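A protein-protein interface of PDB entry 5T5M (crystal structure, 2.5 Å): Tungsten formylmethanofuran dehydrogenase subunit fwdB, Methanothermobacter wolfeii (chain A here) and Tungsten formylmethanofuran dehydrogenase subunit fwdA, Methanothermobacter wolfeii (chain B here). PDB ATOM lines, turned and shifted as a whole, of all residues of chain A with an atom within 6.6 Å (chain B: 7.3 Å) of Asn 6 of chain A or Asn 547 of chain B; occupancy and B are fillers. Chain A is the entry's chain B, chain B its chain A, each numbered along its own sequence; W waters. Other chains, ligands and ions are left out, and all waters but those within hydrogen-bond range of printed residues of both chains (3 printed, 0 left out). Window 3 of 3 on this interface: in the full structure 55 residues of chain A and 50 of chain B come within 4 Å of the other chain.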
ATOM      1  N   VAL A   4      -5.231   9.859   2.249  1.00  0.00           N
ATOM      2  CA  VAL A   4      -3.941  10.281   2.776  1.00  0.00           C
ATOM      3  C   VAL A   4      -3.121  10.769   1.597  1.00  0.00           C
ATOM      4  O   VAL A   4      -2.713   9.975   0.741  1.00  0.00           O
ATOM      5  CB  VAL A   4      -3.220   9.153   3.520  1.00  0.00           C
ATOM      6  CG1 VAL A   4      -1.985   9.707   4.229  1.00  0.00           C
ATOM      7  CG2 VAL A   4      -4.162   8.464   4.496  1.00  0.00           C
ATOM      8  N   LYS A   5      -2.874  12.070   1.556  1.00  0.00           N
ATOM      9  CA  LYS A   5      -2.127  12.700   0.482  1.00  0.00           C
ATOM     10  C   LYS A   5      -0.710  12.998   0.948  1.00  0.00           C
ATOM     11  O   LYS A   5      -0.410  12.988   2.143  1.00  0.00           O
ATOM     12  CB  LYS A   5      -2.815  13.993   0.028  1.00  0.00           C
ATOM     13  CG  LYS A   5      -4.222  13.795  -0.535  1.00  0.00           C
ATOM     14  CD  LYS A   5      -4.803  15.094  -1.099  1.00  0.00           C
ATOM     15  CE  LYS A   5      -6.178  14.883  -1.725  1.00  0.00           C
ATOM     16  NZ  LYS A   5      -6.747  16.139  -2.297  1.00  0.00           N
ATOM     17  N   ASN A   6       0.166  13.261  -0.021  1.00  0.00           N
ATOM     18  CA  ASN A   6       1.576  13.554   0.239  1.00  0.00           C
ATOM     19  C   ASN A   6       2.318  12.366   0.861  1.00  0.00           C
ATOM     20  O   ASN A   6       3.231  12.548   1.672  1.00  0.00           O
ATOM     21  CB  ASN A   6       1.720  14.795   1.123  1.00  0.00           C
ATOM     22  CG  ASN A   6       0.991  15.984   0.564  1.00  0.00           C
ATOM     23  OD1 ASN A   6       1.493  16.674  -0.324  1.00  0.00           O
ATOM     24  ND2 ASN A   6      -0.202  16.239   1.080  1.00  0.00           N
ATOM     25  N   VAL A   7       1.946  11.146   0.476  1.00  0.00           N
ATOM     26  CA  VAL A   7       2.648   9.940   0.915  1.00  0.00           C
ATOM     27  C   VAL A   7       3.894   9.732   0.064  1.00  0.00           C
ATOM     28  O   VAL A   7       3.888   9.975  -1.151  1.00  0.00           O
ATOM     29  CB  VAL A   7       1.722   8.712   0.830  1.00  0.00           C
ATOM     30  CG1 VAL A   7       2.433   7.473   1.366  1.00  0.00           C
ATOM     31  CG2 VAL A   7       0.426   8.956   1.570  1.00  0.00           C
ATOM     32  N   VAL A   8       4.961   9.248   0.696  1.00  0.00           N
ATOM     33  CA  VAL A   8       6.211   8.938   0.017  1.00  0.00           C
ATOM     34  C   VAL A   8       6.214   7.454  -0.328  1.00  0.00           C
ATOM     35  O   VAL A   8       6.003   6.602   0.542  1.00  0.00           O
ATOM     36  CB  VAL A   8       7.429   9.310   0.881  1.00  0.00           C
ATOM     37  CG1 VAL A   8       8.696   9.324   0.008  1.00  0.00           C
ATOM     38  CG2 VAL A   8       7.221  10.664   1.569  1.00  0.00           C
ATOM     39  N   ASP A  17       6.896  11.610  -3.703  1.00  0.00           N
ATOM     40  CA  ASP A  17       6.299  12.072  -2.458  1.00  0.00           C
ATOM     41  C   ASP A  17       4.928  12.708  -2.688  1.00  0.00           C
ATOM     42  O   ASP A  17       4.492  13.556  -1.910  1.00  0.00           O
ATOM     43  CB  ASP A  17       7.241  13.053  -1.764  1.00  0.00           C
ATOM     44  CG  ASP A  17       7.418  14.341  -2.542  1.00  0.00           C
ATOM     45  OD1 ASP A  17       7.410  14.295  -3.795  1.00  0.00           O
ATOM     46  OD2 ASP A  17       7.541  15.406  -1.890  1.00  0.00           O
ATOM     47  N   ASP A  18       4.235  12.303  -3.751  1.00  0.00           N
ATOM     48  CA  ASP A  18       2.914  12.827  -4.085  1.00  0.00           C
ATOM     49  C   ASP A  18       1.878  11.709  -4.164  1.00  0.00           C
ATOM     50  O   ASP A  18       0.879  11.831  -4.876  1.00  0.00           O
ATOM     51  CB  ASP A  18       2.961  13.586  -5.408  1.00  0.00           C
ATOM     52  CG  ASP A  18       3.389  12.695  -6.554  1.00  0.00           C
ATOM     53  OD1 ASP A  18       3.978  11.636  -6.253  1.00  0.00           O
ATOM     54  OD2 ASP A  18       3.137  13.036  -7.733  1.00  0.00           O
ATOM     55  N   ILE A  19       2.109  10.605  -3.467  1.00  0.00           N
ATOM     56  CA  ILE A  19       1.176   9.486  -3.514  1.00  0.00           C
ATOM     57  C   ILE A  19      -0.030   9.808  -2.647  1.00  0.00           C
ATOM     58  O   ILE A  19       0.085  10.444  -1.590  1.00  0.00           O
ATOM     59  CB  ILE A  19       1.856   8.184  -3.057  1.00  0.00           C
ATOM     60  CG1 ILE A  19       3.145   7.923  -3.857  1.00  0.00           C
ATOM     61  CG2 ILE A  19       0.897   7.016  -3.199  1.00  0.00           C
ATOM     62  CD1 ILE A  19       2.969   7.882  -5.359  1.00  0.00           C
ATOM     63  N   ILE A  20      -1.199   9.373  -3.104  1.00  0.00           N
ATOM     64  CA  ILE A  20      -2.438   9.480  -2.350  1.00  0.00           C
ATOM     65  C   ILE A  20      -2.905   8.064  -2.050  1.00  0.00           C
ATOM     66  O   ILE A  20      -3.101   7.262  -2.974  1.00  0.00           O
ATOM     67  CB  ILE A  20      -3.504  10.261  -3.129  1.00  0.00           C
ATOM     68  CG1 ILE A  20      -3.027  11.700  -3.382  1.00  0.00           C
ATOM     69  CG2 ILE A  20      -4.858  10.206  -2.399  1.00  0.00           C
ATOM     70  CD1 ILE A  20      -4.026  12.572  -4.159  1.00  0.00           C
ATOM     71  N   CYS A  21      -3.100   7.760  -0.770  1.00  0.00           N
ATOM     72  CA  CYS A  21      -3.491   6.423  -0.339  1.00  0.00           C
ATOM     73  C   CYS A  21      -4.967   6.392   0.025  1.00  0.00           C
ATOM     74  O   CYS A  21      -5.458   7.264   0.754  1.00  0.00           O
ATOM     75  CB  CYS A  21      -2.647   5.961   0.849  1.00  0.00           C
ATOM     76  SG  CYS A  21      -0.974   5.492   0.359  1.00  0.00           S
ATOM     77  N   ARG A 402      11.076  12.188   4.478  1.00  0.00           N
ATOM     78  CA  ARG A 402      10.635  11.350   5.588  1.00  0.00           C
ATOM     79  C   ARG A 402       9.466  10.466   5.159  1.00  0.00           C
ATOM     80  O   ARG A 402       8.406  10.961   4.767  1.00  0.00           O
ATOM     81  CB  ARG A 402      10.244  12.207   6.789  1.00  0.00           C
ATOM     82  CG  ARG A 402       9.916  11.363   8.015  1.00  0.00           C
ATOM     83  CD  ARG A 402       9.766  12.202   9.271  1.00  0.00           C
ATOM     84  NE  ARG A 402       9.457  11.380  10.436  1.00  0.00           N
ATOM     85  CZ  ARG A 402      10.355  10.716  11.157  1.00  0.00           C
ATOM     86  NH1 ARG A 402      11.650  10.755  10.838  1.00  0.00           N
ATOM     87  NH2 ARG A 402       9.951  10.004  12.202  1.00  0.00           N
ATOM     88  N   LYS A 404       6.277   8.005   5.641  1.00  0.00           N
ATOM     89  CA  LYS A 404       5.122   8.273   6.484  1.00  0.00           C
ATOM     90  C   LYS A 404       4.421   6.987   6.893  1.00  0.00           C
ATOM     91  O   LYS A 404       4.364   6.014   6.139  1.00  0.00           O
ATOM     92  CB  LYS A 404       4.135   9.195   5.774  1.00  0.00           C
ATOM     93  CG  LYS A 404       4.612  10.626   5.737  1.00  0.00           C
ATOM     94  CD  LYS A 404       3.629  11.521   5.022  1.00  0.00           C
ATOM     95  CE  LYS A 404       4.119  12.946   5.016  1.00  0.00           C
ATOM     96  NZ  LYS A 404       3.189  13.842   4.288  1.00  0.00           N
ATOM     97  N   GLU B 537       4.186  28.078  -1.604  1.00  0.00           N
ATOM     98  CA  GLU B 537       3.571  26.792  -1.909  1.00  0.00           C
ATOM     99  C   GLU B 537       3.174  26.711  -3.377  1.00  0.00           C
ATOM    100  O   GLU B 537       3.334  25.662  -4.011  1.00  0.00           O
ATOM    101  CB  GLU B 537       2.363  26.556  -1.010  1.00  0.00           C
ATOM    102  CG  GLU B 537       1.599  25.294  -1.367  1.00  0.00           C
ATOM    103  CD  GLU B 537       0.714  24.796  -0.245  1.00  0.00           C
ATOM    104  OE1 GLU B 537       0.359  23.596  -0.274  1.00  0.00           O
ATOM    105  OE2 GLU B 537       0.377  25.598   0.657  1.00  0.00           O
ATOM    106  N   PHE B 540       6.203  25.770  -5.252  1.00  0.00           N
ATOM    107  CA  PHE B 540       6.550  24.369  -5.049  1.00  0.00           C
ATOM    108  C   PHE B 540       5.766  23.470  -5.991  1.00  0.00           C
ATOM    109  O   PHE B 540       6.321  22.531  -6.574  1.00  0.00           O
ATOM    110  CB  PHE B 540       6.282  23.966  -3.601  1.00  0.00           C
ATOM    111  CG  PHE B 540       7.469  24.111  -2.692  1.00  0.00           C
ATOM    112  CD1 PHE B 540       7.832  25.349  -2.170  1.00  0.00           C
ATOM    113  CD2 PHE B 540       8.199  23.000  -2.330  1.00  0.00           C
ATOM    114  CE1 PHE B 540       8.923  25.465  -1.319  1.00  0.00           C
ATOM    115  CE2 PHE B 540       9.289  23.107  -1.489  1.00  0.00           C
ATOM    116  CZ  PHE B 540       9.654  24.334  -0.983  1.00  0.00           C
ATOM    117  N   LYS B 541       4.471  23.738  -6.151  1.00  0.00           N
ATOM    118  CA  LYS B 541       3.657  22.932  -7.052  1.00  0.00           C
ATOM    119  C   LYS B 541       4.186  22.976  -8.479  1.00  0.00           C
ATOM    120  O   LYS B 541       4.085  21.981  -9.205  1.00  0.00           O
ATOM    121  CB  LYS B 541       2.210  23.419  -7.027  1.00  0.00           C
ATOM    122  CG  LYS B 541       1.581  23.406  -5.654  1.00  0.00           C
ATOM    123  CD  LYS B 541       0.177  23.958  -5.685  1.00  0.00           C
ATOM    124  CE  LYS B 541      -0.408  23.974  -4.305  1.00  0.00           C
ATOM    125  NZ  LYS B 541      -1.716  24.669  -4.270  1.00  0.00           N
ATOM    126  N   TYR B 544       9.379  22.946  -7.821  1.00  0.00           N
ATOM    127  CA  TYR B 544      10.136  22.033  -6.984  1.00  0.00           C
ATOM    128  C   TYR B 544       9.849  20.600  -7.408  1.00  0.00           C
ATOM    129  O   TYR B 544       8.841  20.312  -8.063  1.00  0.00           O
ATOM    130  CB  TYR B 544       9.787  22.230  -5.508  1.00  0.00           C
ATOM    131  CG  TYR B 544      10.779  23.082  -4.732  1.00  0.00           C
ATOM    132  CD1 TYR B 544      11.950  22.527  -4.221  1.00  0.00           C
ATOM    133  CD2 TYR B 544      10.539  24.433  -4.501  1.00  0.00           C
ATOM    134  CE1 TYR B 544      12.858  23.294  -3.504  1.00  0.00           C
ATOM    135  CE2 TYR B 544      11.444  25.215  -3.786  1.00  0.00           C
ATOM    136  CZ  TYR B 544      12.597  24.639  -3.291  1.00  0.00           C
ATOM    137  OH  TYR B 544      13.488  25.405  -2.584  1.00  0.00           O
ATOM    138  N   SER B 545      10.763  19.698  -7.047  1.00  0.00           N
ATOM    139  CA  SER B 545      10.606  18.271  -7.307  1.00  0.00           C
ATOM    140  C   SER B 545      10.021  17.517  -6.121  1.00  0.00           C
ATOM    141  O   SER B 545       9.995  16.284  -6.139  1.00  0.00           O
ATOM    142  CB  SER B 545      11.944  17.659  -7.686  1.00  0.00           C
ATOM    143  OG  SER B 545      12.779  17.584  -6.548  1.00  0.00           O
ATOM    144  N   VAL B 546       9.554  18.232  -5.096  1.00  0.00           N
ATOM    145  CA  VAL B 546       8.951  17.647  -3.910  1.00  0.00           C
ATOM    146  C   VAL B 546       7.681  18.426  -3.593  1.00  0.00           C
ATOM    147  O   VAL B 546       7.521  19.586  -3.976  1.00  0.00           O
ATOM    148  CB  VAL B 546       9.904  17.668  -2.697  1.00  0.00           C
ATOM    149  CG1 VAL B 546      11.138  16.833  -2.965  1.00  0.00           C
ATOM    150  CG2 VAL B 546      10.300  19.108  -2.366  1.00  0.00           C
ATOM    151  N   ASN B 547       6.771  17.776  -2.879  1.00  0.00           N
ATOM    152  CA  ASN B 547       5.536  18.434  -2.482  1.00  0.00           C
ATOM    153  C   ASN B 547       5.779  19.305  -1.253  1.00  0.00           C
ATOM    154  O   ASN B 547       6.553  18.948  -0.357  1.00  0.00           O
ATOM    155  CB  ASN B 547       4.435  17.409  -2.222  1.00  0.00           C
ATOM    156  CG  ASN B 547       3.638  17.082  -3.481  1.00  0.00           C
ATOM    157  OD1 ASN B 547       4.021  17.456  -4.586  1.00  0.00           O
ATOM    158  ND2 ASN B 547       2.524  16.394  -3.315  1.00  0.00           N
ATOM    159  N   PHE B 548       5.129  20.473  -1.243  1.00  0.00           N
ATOM    160  CA  PHE B 548       5.351  21.470  -0.198  1.00  0.00           C
ATOM    161  C   PHE B 548       5.195  20.864   1.197  1.00  0.00           C
ATOM    162  O   PHE B 548       5.986  21.157   2.101  1.00  0.00           O
ATOM    163  CB  PHE B 548       4.376  22.635  -0.418  1.00  0.00           C
ATOM    164  CG  PHE B 548       4.405  23.681   0.663  1.00  0.00           C
ATOM    165  CD1 PHE B 548       5.488  24.530   0.799  1.00  0.00           C
ATOM    166  CD2 PHE B 548       3.336  23.824   1.532  1.00  0.00           C
ATOM    167  CE1 PHE B 548       5.506  25.496   1.793  1.00  0.00           C
ATOM    168  CE2 PHE B 548       3.348  24.788   2.521  1.00  0.00           C
ATOM    169  CZ  PHE B 548       4.427  25.622   2.655  1.00  0.00           C
ATOM    170  N   ALA B 549       4.199  19.989   1.377  1.00  0.00           N
ATOM    171  CA  ALA B 549       3.936  19.409   2.691  1.00  0.00           C
ATOM    172  C   ALA B 549       5.135  18.648   3.244  1.00  0.00           C
ATOM    173  O   ALA B 549       5.306  18.571   4.466  1.00  0.00           O
ATOM    174  CB  ALA B 549       2.724  18.481   2.615  1.00  0.00           C
ATOM    175  N   ASN B 550       5.965  18.071   2.378  1.00  0.00           N
ATOM    176  CA  ASN B 550       7.074  17.229   2.819  1.00  0.00           C
ATOM    177  C   ASN B 550       8.376  18.009   3.022  1.00  0.00           C
ATOM    178  O   ASN B 550       9.354  17.435   3.502  1.00  0.00           O
ATOM    179  CB  ASN B 550       7.276  16.092   1.806  1.00  0.00           C
ATOM    180  CG  ASN B 550       6.082  15.142   1.748  1.00  0.00           C
ATOM    181  OD1 ASN B 550       5.626  14.627   2.770  1.00  0.00           O
ATOM    182  ND2 ASN B 550       5.569  14.918   0.550  1.00  0.00           N
ATOM    183  N   TYR B 551       8.393  19.309   2.727  1.00  0.00           N
ATOM    184  CA  TYR B 551       9.653  20.051   2.724  1.00  0.00           C
ATOM    185  C   TYR B 551      10.185  20.331   4.129  1.00  0.00           C
ATOM    186  O   TYR B 551      11.343  19.982   4.404  1.00  0.00           O
ATOM    187  CB  TYR B 551       9.464  21.334   1.902  1.00  0.00           C
ATOM    188  CG  TYR B 551      10.678  22.217   1.717  1.00  0.00           C
ATOM    189  CD1 TYR B 551      11.591  21.978   0.696  1.00  0.00           C
ATOM    190  CD2 TYR B 551      10.873  23.330   2.526  1.00  0.00           C
ATOM    191  CE1 TYR B 551      12.683  22.809   0.504  1.00  0.00           C
ATOM    192  CE2 TYR B 551      11.961  24.164   2.351  1.00  0.00           C
ATOM    193  CZ  TYR B 551      12.866  23.902   1.338  1.00  0.00           C
ATOM    194  OH  TYR B 551      13.950  24.742   1.170  1.00  0.00           O
ATOM    195  N   PRO B 552       9.425  20.923   5.049  1.00  0.00           N
ATOM    196  CA  PRO B 552      10.017  21.364   6.323  1.00  0.00           C
ATOM    197  C   PRO B 552      10.540  20.213   7.170  1.00  0.00           C
ATOM    198  O   PRO B 552      10.015  19.101   7.141  1.00  0.00           O
ATOM    199  CB  PRO B 552       8.855  22.077   7.029  1.00  0.00           C
ATOM    200  CG  PRO B 552       7.892  22.397   5.953  1.00  0.00           C
ATOM    201  CD  PRO B 552       8.002  21.275   4.968  1.00  0.00           C
HETATM  202  O   HOH W   1       9.577  14.858   4.495  1.00  0.00           O
HETATM  203  O   HOH W   2       7.374  13.511   4.780  1.00  0.00           O
HETATM  204  O   HOH W   3       2.218  19.618  -0.677  1.00  0.00           O
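The side-chain amide oxygen (OD1) of Asn 550 of chain B lies close to the backbone carbonyl oxygen (O) of Asn 6 of chain A (3.4 Å). The side-chain carboxylate of Asp 17 of chain A sits at hydrogen-bond distance from the backbone NH of Asn 547 of chain B, 2.7 Å away. ND2 of Asn 550 of chain B lies within hydrogen-bond range of O of Asp 17 of chain A (3.0 Å). The side-chain amino group (NZ) of Lys 404 of chain A sits at hydrogen-bond distance from the side-chain amide oxygen (OD1) of Asn 550 of chain B, at 3.0 Å. ND2 of Asn 547 of chain B lies within hydrogen-bond range of OD1 of Asn 6 of chain A.
O of Ile 19 of chain A sits at hydrogen-bond distance from N of Asn 6 of chain A (3.2 Å). NZ of Lys 404 of chain A sits at hydrogen-bond distance from O of Asn 6 of chain A, 2.9 Å away.
Among the printed residues, merely in contact across the chains: Asn 6 of chain A with Ala 549 of chain B (3.7 Å), Asp 17 of chain A with Val 546 of chain B (3.3 Å) and Asp 18 of chain A with Asn 547 of chain B (3.5 Å).
Of the printed residues of chain B, Asp 17 of chain A touches Val 546 (3.3 Å), Asn 547 (2.7 Å) and Asn 550 (3.0 Å). Of the printed residues of chain B, Asp 18 of chain A touches Asn 547 (3.5 Å). Of the printed residues of chain B, Lys 404 of chain A touches Asn 550 (3.0 Å). Lys 541 of chain B touches none of the printed residues of chain A. Of the printed residues of chain A, Val 546 of chain B touches Asp 17. Of the printed residues of chain A, Asn 550 of chain B touches Asn 6, Asp 17 and Lys 404. The nearest residue of chain B that does not touch Asn 6 of chain A is Phe 548 of chain B (5.3 Å).
Of the 12 printed residues of chain A, 4 touch a printed residue of chain B. Along chain A the printed residues that touch a printed residue of chain B span positions 6 to 404. Hydrophobic or aromatic side chains of chain B within 4 Å of the printed part of chain A: Val 546 and Ala 549. Among the printed residues, 8 pairs touch across the chains. Among the printed residues, no Asp or Glu carboxylate lies within 4 Å of a Lys or Arg side-chain nitrogen of the other chain.
Water W2 lies within hydrogen-bond range of O of Arg 402 of chain A (2.8 Å) and OD1 of Asn 550 of chain B (2.9 Å). Water W1 lies within hydrogen-bond range of O of Asn 550 of chain B (2.8 Å) and N of Arg 402 of chain A (3.1 Å). Water W3 lies within hydrogen-bond range of the backbone NH of Ala 549 of chain B (2.9 Å), the side-chain amide oxygen of Asn 6 of chain A (3.1 Å) and the backbone NH of Phe 548 of chain B (3.1 Å).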
